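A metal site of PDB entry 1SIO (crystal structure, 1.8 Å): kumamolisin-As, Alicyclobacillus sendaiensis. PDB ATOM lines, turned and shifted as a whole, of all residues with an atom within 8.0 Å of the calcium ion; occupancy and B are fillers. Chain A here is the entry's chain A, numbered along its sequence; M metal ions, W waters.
OD1 of Asp 338 is in hydrogen-bond range of OG1 of Thr 341 (2.9 Å).
The side-chain carboxylate (OD1) of Asp 338 lies within hydrogen-bond range of the backbone NH (N) of Cys 340, 3.1 Å away.
Five residues have an atom within 4 Å of the calcium ion: Asp 316, Ile 317, Gly 334, Gly 336 and Asp 338.
The calcium ion is bound by the side-chain carboxylate of Asp 338 (2.3 Å), the side-chain carboxylate of Asp 316 (2.3 Å), the backbone carbonyl oxygen of Gly 334 (2.3 Å), water W1 (2.3 Å), the backbone carbonyl oxygen of Gly 336 (2.3 Å) and the backbone carbonyl oxygen of Ile 317 (2.4 Å).
The calcium ion has six donor atoms within binding distance.
Water W1 lies within hydrogen-bond range of the backbone carbonyl oxygen (O) of Gly 342 (2.9 Å), the side-chain hydroxyl (OG1) of Thr 341 (2.9 Å), the backbone NH (N) of Ile 317 (3.2 Å) and the backbone NH (N) of Gly 344 (3.5 Å).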
ATOM      1  N   VAL A 207       5.580 -14.344  -0.723  1.00  0.00           N
ATOM      2  CA  VAL A 207       5.564 -15.108   0.507  1.00  0.00           C
ATOM      3  C   VAL A 207       4.419 -14.666   1.426  1.00  0.00           C
ATOM      4  O   VAL A 207       4.218 -13.445   1.546  1.00  0.00           O
ATOM      5  CB  VAL A 207       6.866 -14.948   1.296  1.00  0.00           C
ATOM      6  CG1 VAL A 207       6.862 -15.715   2.618  1.00  0.00           C
ATOM      7  CG2 VAL A 207       8.080 -15.442   0.509  1.00  0.00           C
ATOM      8  N   HIS A 315       5.565 -22.333 -10.646  1.00  0.00           N
ATOM      9  CA  HIS A 315       5.540 -20.896 -10.562  1.00  0.00           C
ATOM     10  C   HIS A 315       6.447 -20.451  -9.404  1.00  0.00           C
ATOM     11  O   HIS A 315       6.172 -20.704  -8.210  1.00  0.00           O
ATOM     12  CB  HIS A 315       4.101 -20.418 -10.379  1.00  0.00           C
ATOM     13  CG  HIS A 315       4.188 -18.918 -10.313  1.00  0.00           C
ATOM     14  ND1 HIS A 315       4.199 -18.194  -9.138  1.00  0.00           N
ATOM     15  CD2 HIS A 315       4.285 -18.051 -11.367  1.00  0.00           C
ATOM     16  CE1 HIS A 315       4.294 -16.913  -9.484  1.00  0.00           C
ATOM     17  NE2 HIS A 315       4.344 -16.797 -10.791  1.00  0.00           N
ATOM     18  N   ASP A 316       7.542 -19.812  -9.750  1.00  0.00           N
ATOM     19  CA  ASP A 316       8.599 -19.450  -8.817  1.00  0.00           C
ATOM     20  C   ASP A 316       8.161 -18.239  -8.015  1.00  0.00           C
ATOM     21  O   ASP A 316       7.795 -17.219  -8.571  1.00  0.00           O
ATOM     22  CB  ASP A 316       9.885 -19.177  -9.579  1.00  0.00           C
ATOM     23  CG  ASP A 316      11.114 -19.020  -8.719  1.00  0.00           C
ATOM     24  OD1 ASP A 316      11.039 -19.197  -7.488  1.00  0.00           O
ATOM     25  OD2 ASP A 316      12.185 -18.721  -9.276  1.00  0.00           O
ATOM     26  N   ILE A 317       8.185 -18.349  -6.695  1.00  0.00           N
ATOM     27  CA  ILE A 317       7.930 -17.165  -5.874  1.00  0.00           C
ATOM     28  C   ILE A 317       9.323 -16.576  -5.531  1.00  0.00           C
ATOM     29  O   ILE A 317      10.177 -17.331  -5.051  1.00  0.00           O
ATOM     30  CB  ILE A 317       7.146 -17.421  -4.609  1.00  0.00           C
ATOM     31  CG1 ILE A 317       5.645 -17.693  -4.909  1.00  0.00           C
ATOM     32  CG2 ILE A 317       7.235 -16.270  -3.584  1.00  0.00           C
ATOM     33  CD1 ILE A 317       5.385 -19.199  -5.026  1.00  0.00           C
ATOM     34  N   THR A 318       9.458 -15.256  -5.787  1.00  0.00           N
ATOM     35  CA  THR A 318      10.809 -14.729  -5.582  1.00  0.00           C
ATOM     36  C   THR A 318      10.847 -13.567  -4.598  1.00  0.00           C
ATOM     37  O   THR A 318      11.916 -13.078  -4.207  1.00  0.00           O
ATOM     38  CB  THR A 318      11.413 -14.172  -6.881  1.00  0.00           C
ATOM     39  OG1 THR A 318      10.373 -13.326  -7.404  1.00  0.00           O
ATOM     40  CG2 THR A 318      11.733 -15.227  -7.915  1.00  0.00           C
ATOM     41  N   GLU A 319       9.682 -13.115  -4.189  1.00  0.00           N
ATOM     42  CA  GLU A 319       9.640 -11.892  -3.355  1.00  0.00           C
ATOM     43  C   GLU A 319       8.958 -12.175  -2.039  1.00  0.00           C
ATOM     44  O   GLU A 319       7.887 -12.820  -1.971  1.00  0.00           O
ATOM     45  CB  GLU A 319       8.934 -10.857  -4.195  1.00  0.00           C
ATOM     46  CG  GLU A 319       8.820  -9.413  -3.782  1.00  0.00           C
ATOM     47  CD  GLU A 319       7.771  -8.585  -4.518  1.00  0.00           C
ATOM     48  OE1 GLU A 319       7.132  -9.042  -5.497  1.00  0.00           O
ATOM     49  OE2 GLU A 319       7.555  -7.418  -4.118  1.00  0.00           O
ATOM     50  N   GLN A 332      14.372 -15.741   3.333  1.00  0.00           N
ATOM     51  CA  GLN A 332      13.833 -14.977   2.212  1.00  0.00           C
ATOM     52  C   GLN A 332      13.628 -15.738   0.916  1.00  0.00           C
ATOM     53  O   GLN A 332      14.369 -16.633   0.480  1.00  0.00           O
ATOM     54  CB  GLN A 332      14.834 -13.857   1.903  1.00  0.00           C
ATOM     55  CG  GLN A 332      14.202 -12.586   1.373  1.00  0.00           C
ATOM     56  CD  GLN A 332      15.076 -11.902   0.335  1.00  0.00           C
ATOM     57  OE1 GLN A 332      14.568 -11.306  -0.608  1.00  0.00           O
ATOM     58  NE2 GLN A 332      16.385 -12.016   0.549  1.00  0.00           N
ATOM     59  N   ALA A 333      12.594 -15.352   0.196  1.00  0.00           N
ATOM     60  CA  ALA A 333      12.378 -15.982  -1.101  1.00  0.00           C
ATOM     61  C   ALA A 333      13.350 -15.501  -2.159  1.00  0.00           C
ATOM     62  O   ALA A 333      13.944 -14.430  -2.058  1.00  0.00           O
ATOM     63  CB  ALA A 333      10.937 -15.692  -1.508  1.00  0.00           C
ATOM     64  N   GLY A 334      13.559 -16.279  -3.223  1.00  0.00           N
ATOM     65  CA  GLY A 334      14.437 -15.872  -4.300  1.00  0.00           C
ATOM     66  C   GLY A 334      14.313 -16.824  -5.483  1.00  0.00           C
ATOM     67  O   GLY A 334      13.443 -17.704  -5.417  1.00  0.00           O
ATOM     68  N   PRO A 335      15.118 -16.663  -6.516  1.00  0.00           N
ATOM     69  CA  PRO A 335      15.030 -17.527  -7.711  1.00  0.00           C
ATOM     70  C   PRO A 335      15.172 -18.997  -7.348  1.00  0.00           C
ATOM     71  O   PRO A 335      15.979 -19.410  -6.509  1.00  0.00           O
ATOM     72  CB  PRO A 335      16.207 -17.031  -8.572  1.00  0.00           C
ATOM     73  CG  PRO A 335      16.284 -15.577  -8.172  1.00  0.00           C
ATOM     74  CD  PRO A 335      16.184 -15.645  -6.664  1.00  0.00           C
ATOM     75  N   GLY A 336      14.350 -19.850  -8.027  1.00  0.00           N
ATOM     76  CA  GLY A 336      14.407 -21.278  -7.713  1.00  0.00           C
ATOM     77  C   GLY A 336      13.893 -21.665  -6.356  1.00  0.00           C
ATOM     78  O   GLY A 336      13.048 -20.965  -5.783  1.00  0.00           O
ATOM     79  N   TRP A 337      14.400 -22.802  -5.843  1.00  0.00           N
ATOM     80  CA  TRP A 337      13.977 -23.233  -4.491  1.00  0.00           C
ATOM     81  C   TRP A 337      14.385 -22.243  -3.399  1.00  0.00           C
ATOM     82  O   TRP A 337      15.537 -21.785  -3.364  1.00  0.00           O
ATOM     83  CB  TRP A 337      14.535 -24.606  -4.158  1.00  0.00           C
ATOM     84  CG  TRP A 337      14.062 -25.145  -2.819  1.00  0.00           C
ATOM     85  CD1 TRP A 337      13.063 -26.083  -2.720  1.00  0.00           C
ATOM     86  CD2 TRP A 337      14.465 -24.892  -1.468  1.00  0.00           C
ATOM     87  NE1 TRP A 337      12.839 -26.402  -1.395  1.00  0.00           N
ATOM     88  CE2 TRP A 337      13.681 -25.673  -0.608  1.00  0.00           C
ATOM     89  CE3 TRP A 337      15.406 -24.060  -0.854  1.00  0.00           C
ATOM     90  CZ2 TRP A 337      13.796 -25.679   0.761  1.00  0.00           C
ATOM     91  CZ3 TRP A 337      15.508 -24.071   0.515  1.00  0.00           C
ATOM     92  CH2 TRP A 337      14.733 -24.856   1.373  1.00  0.00           C
ATOM     93  N   ASP A 338      13.457 -21.919  -2.481  1.00  0.00           N
ATOM     94  CA  ASP A 338      13.840 -21.120  -1.295  1.00  0.00           C
ATOM     95  C   ASP A 338      13.206 -21.678  -0.023  1.00  0.00           C
ATOM     96  O   ASP A 338      12.276 -22.494  -0.119  1.00  0.00           O
ATOM     97  CB  ASP A 338      13.515 -19.654  -1.538  1.00  0.00           C
ATOM     98  CG  ASP A 338      12.077 -19.389  -1.890  1.00  0.00           C
ATOM     99  OD1 ASP A 338      11.240 -19.659  -1.010  1.00  0.00           O
ATOM    100  OD2 ASP A 338      11.823 -18.903  -3.006  1.00  0.00           O
ATOM    101  N   PRO A 339      13.632 -21.276   1.169  1.00  0.00           N
ATOM    102  CA  PRO A 339      13.085 -21.828   2.420  1.00  0.00           C
ATOM    103  C   PRO A 339      11.781 -21.143   2.854  1.00  0.00           C
ATOM    104  O   PRO A 339      11.386 -21.196   4.028  1.00  0.00           O
ATOM    105  CB  PRO A 339      14.224 -21.597   3.409  1.00  0.00           C
ATOM    106  CG  PRO A 339      15.376 -21.095   2.574  1.00  0.00           C
ATOM    107  CD  PRO A 339      14.716 -20.287   1.472  1.00  0.00           C
ATOM    108  N   CYS A 340      11.088 -20.454   1.953  1.00  0.00           N
ATOM    109  CA  CYS A 340       9.778 -19.903   2.286  1.00  0.00           C
ATOM    110  C   CYS A 340       8.647 -20.605   1.506  1.00  0.00           C
ATOM    111  O   CYS A 340       7.531 -20.766   2.004  1.00  0.00           O
ATOM    112  CB  CYS A 340       9.605 -18.409   1.935  1.00  0.00           C
ATOM    113  SG  CYS A 340      10.851 -17.343   2.763  1.00  0.00           S
ATOM    114  N   THR A 341       8.975 -20.946   0.258  1.00  0.00           N
ATOM    115  CA  THR A 341       7.975 -21.426  -0.687  1.00  0.00           C
ATOM    116  C   THR A 341       8.470 -22.646  -1.468  1.00  0.00           C
ATOM    117  O   THR A 341       7.783 -23.109  -2.367  1.00  0.00           O
ATOM    118  CB  THR A 341       7.555 -20.344  -1.712  1.00  0.00           C
ATOM    119  OG1 THR A 341       8.717 -19.915  -2.391  1.00  0.00           O
ATOM    120  CG2 THR A 341       6.925 -19.132  -0.999  1.00  0.00           C
ATOM    121  N   GLY A 342       9.616 -23.224  -1.155  1.00  0.00           N
ATOM    122  CA  GLY A 342      10.097 -24.386  -1.917  1.00  0.00           C
ATOM    123  C   GLY A 342      10.283 -24.078  -3.367  1.00  0.00           C
ATOM    124  O   GLY A 342      10.723 -22.974  -3.686  1.00  0.00           O
ATOM    125  N   LEU A 343       9.924 -25.056  -4.210  1.00  0.00           N
ATOM    126  CA  LEU A 343       9.938 -24.915  -5.652  1.00  0.00           C
ATOM    127  C   LEU A 343       8.897 -23.919  -6.131  1.00  0.00           C
ATOM    128  O   LEU A 343       8.905 -23.454  -7.279  1.00  0.00           O
ATOM    129  CB  LEU A 343       9.701 -26.309  -6.328  1.00  0.00           C
ATOM    130  CG  LEU A 343      10.705 -27.398  -6.007  1.00  0.00           C
ATOM    131  CD1 LEU A 343      10.295 -28.781  -6.551  1.00  0.00           C
ATOM    132  CD2 LEU A 343      12.077 -27.060  -6.595  1.00  0.00           C
ATOM    133  N   GLY A 344       7.925 -23.525  -5.281  1.00  0.00           N
ATOM    134  CA  GLY A 344       6.960 -22.560  -5.843  1.00  0.00           C
ATOM    135  C   GLY A 344       5.567 -23.178  -5.848  1.00  0.00           C
ATOM    136  O   GLY A 344       5.388 -24.202  -5.185  1.00  0.00           O
ATOM    137  N   SER A 345       4.605 -22.575  -6.526  1.00  0.00           N
ATOM    138  CA  SER A 345       3.262 -23.119  -6.674  1.00  0.00           C
ATOM    139  C   SER A 345       3.268 -24.073  -7.876  1.00  0.00           C
ATOM    140  O   SER A 345       3.816 -23.670  -8.919  1.00  0.00           O
ATOM    141  CB  SER A 345       2.270 -21.984  -6.815  1.00  0.00           C
ATOM    142  OG  SER A 345       2.454 -21.132  -7.939  1.00  0.00           O
HETATM  143 CA    CA M   1      11.630 -19.171  -5.273  1.00  0.00          CA
HETATM  144  O   HOH W   1       9.797 -20.591  -4.987  1.00  0.00           O
